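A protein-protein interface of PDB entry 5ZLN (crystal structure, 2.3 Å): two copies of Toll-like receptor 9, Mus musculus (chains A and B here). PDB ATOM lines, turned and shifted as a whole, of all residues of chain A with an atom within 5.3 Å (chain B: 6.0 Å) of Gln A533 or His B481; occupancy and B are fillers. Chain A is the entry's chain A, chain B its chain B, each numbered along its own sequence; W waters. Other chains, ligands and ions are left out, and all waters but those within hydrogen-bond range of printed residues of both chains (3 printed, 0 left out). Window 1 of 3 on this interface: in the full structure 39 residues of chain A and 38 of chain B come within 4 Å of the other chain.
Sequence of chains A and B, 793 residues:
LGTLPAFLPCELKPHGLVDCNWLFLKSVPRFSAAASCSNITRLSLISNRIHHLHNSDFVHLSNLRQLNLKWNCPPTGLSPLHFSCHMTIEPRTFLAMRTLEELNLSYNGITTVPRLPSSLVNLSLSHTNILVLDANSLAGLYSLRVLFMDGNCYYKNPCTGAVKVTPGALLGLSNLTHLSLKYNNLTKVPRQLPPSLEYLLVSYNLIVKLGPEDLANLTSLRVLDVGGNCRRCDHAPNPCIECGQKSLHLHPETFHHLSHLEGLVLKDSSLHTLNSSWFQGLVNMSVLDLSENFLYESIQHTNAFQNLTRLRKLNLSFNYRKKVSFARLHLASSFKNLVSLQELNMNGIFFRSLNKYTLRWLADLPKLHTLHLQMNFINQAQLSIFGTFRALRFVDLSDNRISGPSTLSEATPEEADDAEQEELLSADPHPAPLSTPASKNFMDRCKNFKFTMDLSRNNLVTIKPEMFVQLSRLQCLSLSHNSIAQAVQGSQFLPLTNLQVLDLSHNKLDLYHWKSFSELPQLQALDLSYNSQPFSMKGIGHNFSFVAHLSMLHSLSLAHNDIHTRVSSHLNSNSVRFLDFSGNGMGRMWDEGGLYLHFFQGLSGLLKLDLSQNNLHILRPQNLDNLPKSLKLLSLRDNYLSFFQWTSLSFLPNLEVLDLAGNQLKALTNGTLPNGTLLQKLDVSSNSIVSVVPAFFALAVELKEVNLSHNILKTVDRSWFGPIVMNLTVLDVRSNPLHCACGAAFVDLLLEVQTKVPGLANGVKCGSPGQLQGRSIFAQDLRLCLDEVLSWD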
ATOM      1  N   LYS A 508       0.347   6.345   0.884  1.00  0.00           N
ATOM      2  CA  LYS A 508       1.186   6.627   2.040  1.00  0.00           C
ATOM      3  C   LYS A 508       2.257   5.551   2.229  1.00  0.00           C
ATOM      4  O   LYS A 508       2.530   5.092   3.346  1.00  0.00           O
ATOM      5  CB  LYS A 508       0.318   6.769   3.294  1.00  0.00           C
ATOM      6  CG  LYS A 508      -0.637   7.953   3.195  1.00  0.00           C
ATOM      7  CD  LYS A 508      -1.661   7.982   4.316  1.00  0.00           C
ATOM      8  CE  LYS A 508      -2.574   9.195   4.188  1.00  0.00           C
ATOM      9  NZ  LYS A 508      -3.296   9.423   5.471  1.00  0.00           N
ATOM     10  N   ASN A 531       3.239  10.533  -2.251  1.00  0.00           N
ATOM     11  CA  ASN A 531       3.344   9.718  -1.071  1.00  0.00           C
ATOM     12  C   ASN A 531       4.145  10.475   0.005  1.00  0.00           C
ATOM     13  O   ASN A 531       5.080   9.947   0.595  1.00  0.00           O
ATOM     14  CB  ASN A 531       3.999   8.362  -1.418  1.00  0.00           C
ATOM     15  CG  ASN A 531       3.055   7.459  -2.181  1.00  0.00           C
ATOM     16  OD1 ASN A 531       2.847   7.648  -3.383  1.00  0.00           O
ATOM     17  ND2 ASN A 531       2.483   6.493  -1.502  1.00  0.00           N
ATOM     18  N   SER A 532       3.739  11.704   0.278  1.00  0.00           N
ATOM     19  CA  SER A 532       4.563  12.616   1.068  1.00  0.00           C
ATOM     20  C   SER A 532       4.488  12.403   2.575  1.00  0.00           C
ATOM     21  O   SER A 532       5.436  12.695   3.303  1.00  0.00           O
ATOM     22  CB  SER A 532       4.154  14.050   0.759  1.00  0.00           C
ATOM     23  OG  SER A 532       2.871  14.309   1.274  1.00  0.00           O
ATOM     24  N   GLN A 533       3.373  11.896   3.055  1.00  0.00           N
ATOM     25  CA  GLN A 533       3.136  11.905   4.487  1.00  0.00           C
ATOM     26  C   GLN A 533       4.289  11.270   5.297  1.00  0.00           C
ATOM     27  O   GLN A 533       4.739  11.842   6.297  1.00  0.00           O
ATOM     28  CB  GLN A 533       1.785  11.268   4.838  1.00  0.00           C
ATOM     29  CG  GLN A 533       1.476  11.317   6.329  1.00  0.00           C
ATOM     30  CD  GLN A 533       0.058  10.893   6.655  1.00  0.00           C
ATOM     31  OE1 GLN A 533      -0.908  11.380   6.028  1.00  0.00           O
ATOM     32  NE2 GLN A 533      -0.084   9.985   7.650  1.00  0.00           N
ATOM     33  N   PRO A 534       4.795  10.107   4.861  1.00  0.00           N
ATOM     34  CA  PRO A 534       5.887   9.529   5.677  1.00  0.00           C
ATOM     35  C   PRO A 534       7.133  10.385   5.660  1.00  0.00           C
ATOM     36  O   PRO A 534       7.800  10.479   6.666  1.00  0.00           O
ATOM     37  CB  PRO A 534       6.149   8.175   5.020  1.00  0.00           C
ATOM     38  CG  PRO A 534       4.880   7.862   4.291  1.00  0.00           C
ATOM     39  CD  PRO A 534       4.398   9.203   3.770  1.00  0.00           C
ATOM     40  N   PHE A 535       7.425  11.032   4.529  1.00  0.00           N
ATOM     41  CA  PHE A 535       8.626  11.850   4.414  1.00  0.00           C
ATOM     42  C   PHE A 535       8.556  13.119   5.283  1.00  0.00           C
ATOM     43  O   PHE A 535       9.580  13.741   5.535  1.00  0.00           O
ATOM     44  CB  PHE A 535       8.874  12.233   2.971  1.00  0.00           C
ATOM     45  CG  PHE A 535       9.354  11.109   2.113  1.00  0.00           C
ATOM     46  CD1 PHE A 535      10.666  10.651   2.210  1.00  0.00           C
ATOM     47  CD2 PHE A 535       8.513  10.523   1.174  1.00  0.00           C
ATOM     48  CE1 PHE A 535      11.105   9.610   1.417  1.00  0.00           C
ATOM     49  CE2 PHE A 535       8.955   9.487   0.364  1.00  0.00           C
ATOM     50  CZ  PHE A 535      10.253   9.024   0.496  1.00  0.00           C
ATOM     51  N   SER A 536       7.361  13.487   5.722  1.00  0.00           N
ATOM     52  CA  SER A 536       7.145  14.649   6.590  1.00  0.00           C
ATOM     53  C   SER A 536       7.281  14.315   8.074  1.00  0.00           C
ATOM     54  O   SER A 536       7.219  15.230   8.897  1.00  0.00           O
ATOM     55  CB  SER A 536       5.745  15.279   6.344  1.00  0.00           C
ATOM     56  OG  SER A 536       5.471  15.408   4.942  1.00  0.00           O
ATOM     57  N   MET A 537       7.452  13.033   8.435  1.00  0.00           N
ATOM     58  CA  MET A 537       7.728  12.649   9.837  1.00  0.00           C
ATOM     59  C   MET A 537       9.122  13.086  10.278  1.00  0.00           C
ATOM     60  O   MET A 537      10.120  12.528   9.825  1.00  0.00           O
ATOM     61  CB  MET A 537       7.643  11.139  10.026  1.00  0.00           C
ATOM     62  CG  MET A 537       6.254  10.548   9.899  1.00  0.00           C
ATOM     63  SD  MET A 537       6.325   8.740   9.800  1.00  0.00           S
ATOM     64  CE  MET A 537       5.025   8.265  10.911  1.00  0.00           C
ATOM     65  N   ASP B 399       1.057  10.450  13.966  1.00  0.00           N
ATOM     66  CA  ASP B 399       2.117   9.684  13.266  1.00  0.00           C
ATOM     67  C   ASP B 399       2.340   8.294  13.880  1.00  0.00           C
ATOM     68  O   ASP B 399       3.458   7.921  14.247  1.00  0.00           O
ATOM     69  CB  ASP B 399       3.429  10.484  13.226  1.00  0.00           C
ATOM     70  CG  ASP B 399       3.422  11.595  12.165  1.00  0.00           C
ATOM     71  OD1 ASP B 399       3.179  11.310  10.963  1.00  0.00           O
ATOM     72  OD2 ASP B 399       3.710  12.735  12.547  1.00  0.00           O
ATOM     73  N   SER B 456      -3.986  12.519  14.627  1.00  0.00           N
ATOM     74  CA  SER B 456      -3.766  12.762  13.201  1.00  0.00           C
ATOM     75  C   SER B 456      -2.676  11.850  12.685  1.00  0.00           C
ATOM     76  O   SER B 456      -1.887  11.355  13.463  1.00  0.00           O
ATOM     77  CB  SER B 456      -3.364  14.232  12.955  1.00  0.00           C
ATOM     78  OG  SER B 456      -2.095  14.485  13.530  1.00  0.00           O
ATOM     79  N   ARG B 457      -2.639  11.622  11.381  1.00  0.00           N
ATOM     80  CA  ARG B 457      -1.601  10.796  10.762  1.00  0.00           C
ATOM     81  C   ARG B 457      -1.557   9.419  11.400  1.00  0.00           C
ATOM     82  O   ARG B 457      -0.513   8.931  11.776  1.00  0.00           O
ATOM     83  CB  ARG B 457      -0.228  11.492  10.798  1.00  0.00           C
ATOM     84  CG  ARG B 457      -0.201  12.816  10.041  1.00  0.00           C
ATOM     85  CD  ARG B 457       0.700  13.854  10.699  1.00  0.00           C
ATOM     86  NE  ARG B 457       0.345  15.196  10.258  1.00  0.00           N
ATOM     87  CZ  ARG B 457       0.749  15.753   9.112  1.00  0.00           C
ATOM     88  NH1 ARG B 457       1.542  15.100   8.217  1.00  0.00           N
ATOM     89  NH2 ARG B 457       0.318  16.989   8.841  1.00  0.00           N
ATOM     90  N   ASN B 458      -2.720   8.798  11.497  1.00  0.00           N
ATOM     91  CA  ASN B 458      -2.847   7.408  11.885  1.00  0.00           C
ATOM     92  C   ASN B 458      -3.521   6.656  10.743  1.00  0.00           C
ATOM     93  O   ASN B 458      -3.574   7.170   9.639  1.00  0.00           O
ATOM     94  CB  ASN B 458      -3.578   7.301  13.224  1.00  0.00           C
ATOM     95  CG  ASN B 458      -2.626   7.499  14.405  1.00  0.00           C
ATOM     96  OD1 ASN B 458      -2.047   6.526  14.900  1.00  0.00           O
ATOM     97  ND2 ASN B 458      -2.434   8.764  14.841  1.00  0.00           N
ATOM     98  N   LEU B 479      -8.427  14.172  14.062  1.00  0.00           N
ATOM     99  CA  LEU B 479      -8.296  12.961  13.277  1.00  0.00           C
ATOM    100  C   LEU B 479      -7.787  13.281  11.876  1.00  0.00           C
ATOM    101  O   LEU B 479      -8.063  12.555  10.915  1.00  0.00           O
ATOM    102  CB  LEU B 479      -9.646  12.258  13.199  1.00  0.00           C
ATOM    103  CG  LEU B 479     -10.217  11.742  14.511  1.00  0.00           C
ATOM    104  CD1 LEU B 479     -11.668  11.343  14.330  1.00  0.00           C
ATOM    105  CD2 LEU B 479      -9.403  10.559  14.998  1.00  0.00           C
ATOM    106  N   SER B 480      -7.030  14.353  11.745  1.00  0.00           N
ATOM    107  CA  SER B 480      -6.711  14.828  10.396  1.00  0.00           C
ATOM    108  C   SER B 480      -5.697  13.903   9.800  1.00  0.00           C
ATOM    109  O   SER B 480      -5.027  13.176  10.515  1.00  0.00           O
ATOM    110  CB  SER B 480      -6.189  16.291  10.385  1.00  0.00           C
ATOM    111  OG  SER B 480      -4.838  16.349  10.750  1.00  0.00           O
ATOM    112  N   HIS B 481      -5.616  13.897   8.483  1.00  0.00           N
ATOM    113  CA  HIS B 481      -4.588  13.138   7.783  1.00  0.00           C
ATOM    114  C   HIS B 481      -4.641  11.645   8.098  1.00  0.00           C
ATOM    115  O   HIS B 481      -3.612  10.992   8.248  1.00  0.00           O
ATOM    116  CB  HIS B 481      -3.203  13.688   8.124  1.00  0.00           C
ATOM    117  CG  HIS B 481      -2.877  15.021   7.510  1.00  0.00           C
ATOM    118  ND1 HIS B 481      -3.034  16.223   8.194  1.00  0.00           N
ATOM    119  CD2 HIS B 481      -2.340  15.336   6.304  1.00  0.00           C
ATOM    120  CE1 HIS B 481      -2.622  17.217   7.423  1.00  0.00           C
ATOM    121  NE2 HIS B 481      -2.197  16.708   6.274  1.00  0.00           N
ATOM    122  N   ASN B 482      -5.851  11.110   8.208  1.00  0.00           N
ATOM    123  CA  ASN B 482      -6.048   9.689   8.347  1.00  0.00           C
ATOM    124  C   ASN B 482      -6.557   9.218   6.982  1.00  0.00           C
ATOM    125  O   ASN B 482      -6.247   9.851   5.971  1.00  0.00           O
ATOM    126  CB  ASN B 482      -7.003   9.416   9.519  1.00  0.00           C
ATOM    127  CG  ASN B 482      -6.269   9.293  10.847  1.00  0.00           C
ATOM    128  OD1 ASN B 482      -5.940   8.194  11.240  1.00  0.00           O
ATOM    129  ND2 ASN B 482      -6.019  10.421  11.550  1.00  0.00           N
ATOM    130  N   SER B 483      -7.303   8.118   6.909  1.00  0.00           N
ATOM    131  CA  SER B 483      -7.805   7.624   5.623  1.00  0.00           C
ATOM    132  C   SER B 483      -9.316   7.359   5.743  1.00  0.00           C
ATOM    133  O   SER B 483      -9.856   6.397   5.177  1.00  0.00           O
ATOM    134  CB  SER B 483      -7.046   6.361   5.235  1.00  0.00           C
ATOM    135  OG  SER B 483      -5.651   6.636   5.115  1.00  0.00           O
ATOM    136  N   LEU B 504     -11.138  17.179  10.958  1.00  0.00           N
ATOM    137  CA  LEU B 504     -11.236  15.980  10.102  1.00  0.00           C
ATOM    138  C   LEU B 504     -10.562  16.220   8.756  1.00  0.00           C
ATOM    139  O   LEU B 504     -10.804  15.491   7.808  1.00  0.00           O
ATOM    140  CB  LEU B 504     -12.696  15.548   9.939  1.00  0.00           C
ATOM    141  CG  LEU B 504     -13.197  14.654  11.093  1.00  0.00           C
ATOM    142  CD1 LEU B 504     -14.712  14.613  11.241  1.00  0.00           C
ATOM    143  CD2 LEU B 504     -12.639  13.240  10.924  1.00  0.00           C
ATOM    144  N   SER B 505      -9.686  17.226   8.689  1.00  0.00           N
ATOM    145  CA  SER B 505      -9.093  17.593   7.414  1.00  0.00           C
ATOM    146  C   SER B 505      -8.230  16.469   6.836  1.00  0.00           C
ATOM    147  O   SER B 505      -7.715  15.606   7.558  1.00  0.00           O
ATOM    148  CB  SER B 505      -8.271  18.891   7.543  1.00  0.00           C
ATOM    149  OG  SER B 505      -7.146  18.706   8.382  1.00  0.00           O
ATOM    150  N   HIS B 506      -8.091  16.478   5.516  1.00  0.00           N
ATOM    151  CA  HIS B 506      -7.251  15.486   4.834  1.00  0.00           C
ATOM    152  C   HIS B 506      -7.722  14.031   5.108  1.00  0.00           C
ATOM    153  O   HIS B 506      -6.951  13.187   5.528  1.00  0.00           O
ATOM    154  CB  HIS B 506      -5.769  15.687   5.215  1.00  0.00           C
ATOM    155  CG  HIS B 506      -5.184  17.000   4.764  1.00  0.00           C
ATOM    156  ND1 HIS B 506      -4.578  17.169   3.528  1.00  0.00           N
ATOM    157  CD2 HIS B 506      -5.048  18.182   5.415  1.00  0.00           C
ATOM    158  CE1 HIS B 506      -4.123  18.408   3.435  1.00  0.00           C
ATOM    159  NE2 HIS B 506      -4.389  19.042   4.562  1.00  0.00           N
ATOM    160  N   ASN B 507      -9.005  13.782   4.882  1.00  0.00           N
ATOM    161  CA  ASN B 507      -9.559  12.424   4.873  1.00  0.00           C
ATOM    162  C   ASN B 507     -10.368  12.209   3.576  1.00  0.00           C
ATOM    163  O   ASN B 507     -10.158  12.931   2.589  1.00  0.00           O
ATOM    164  CB  ASN B 507     -10.385  12.197   6.148  1.00  0.00           C
ATOM    165  CG  ASN B 507      -9.520  12.015   7.384  1.00  0.00           C
ATOM    166  OD1 ASN B 507      -8.901  10.973   7.545  1.00  0.00           O
ATOM    167  ND2 ASN B 507      -9.459  13.040   8.259  1.00  0.00           N
HETATM  168  O   HOH W   1      -2.232   8.180   7.736  1.00  0.00           O
HETATM  169  O   HOH W   2       3.781  12.902   8.565  1.00  0.00           O
HETATM  170  O   HOH W   3       2.531   9.413   9.432  1.00  0.00           O
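The backbone carbonyl oxygen (O) of Asn B482 is in hydrogen-bond range of the side-chain amino group (NZ) of Lys A508.
O of His B481 sits at hydrogen-bond distance from NZ of Lys A508, at 3.2 Å.
O of Asn B458 sits close to OD1 of Asn B482 (3.0 Å).
A ring nitrogen (ND1) of His B481 sits at hydrogen-bond distance from the side-chain hydroxyl of Ser B480 (3.1 Å).
N of His B481 lies close to O of His B506, at 3.3 Å.
N of Asp B399 is in hydrogen-bond range of O of Ser B456 (3.1 Å).
The backbone NH (N) of Arg B457 lies close to the backbone carbonyl oxygen (O) of His B481 (3.3 Å).
The backbone NH (N) of Asp B399 sits at hydrogen-bond distance from the backbone carbonyl oxygen (O) of Arg B457, 3.1 Å away.
Ser B483 touches Lys A508.
Gln A533 touches Arg B457.
Gln A533 touches His B481.
Met A537 touches Asp B399.
Printed residues of chain B within 4 Å of Gln A533: Arg B457 and His B481.
Of the printed residues of chain B, Met A537 touches Asp B399.
Printed residues of chain A within 4 Å of Asn B482: Lys A508.
Of the printed residues of chain A, Asp B399 touches Met A537.
Of the printed residues of chain A, Ser B483 touches Lys A508 (3.7 Å).
Hydrophobic or aromatic side chains of chain A that line the printed part of chain B: Met A537.
No position is printed for both chains.
Of the 6 pairs that touch across the chains among the printed residues, none has its exchanged pair printed and touching as well.
Water W3 lies within hydrogen-bond range of OD1 of Asp B399 and NE2 of Gln A533.
Water W1 lies within hydrogen-bond range of the backbone carbonyl oxygen of Asn B458 (2.5 Å), the side-chain amino group of Lys A508 (2.8 Å), the side-chain amide nitrogen of Gln A533 (2.8 Å) and the backbone carbonyl oxygen of His B481 (3.2 Å).
Water W2 lies within hydrogen-bond range of the backbone carbonyl oxygen (O) of Gln A533 (2.7 Å), the side-chain carboxylate (OD1) of Asp B399 (2.9 Å) and the guanidinium group (NH1) of Arg B457 (3.2 Å).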
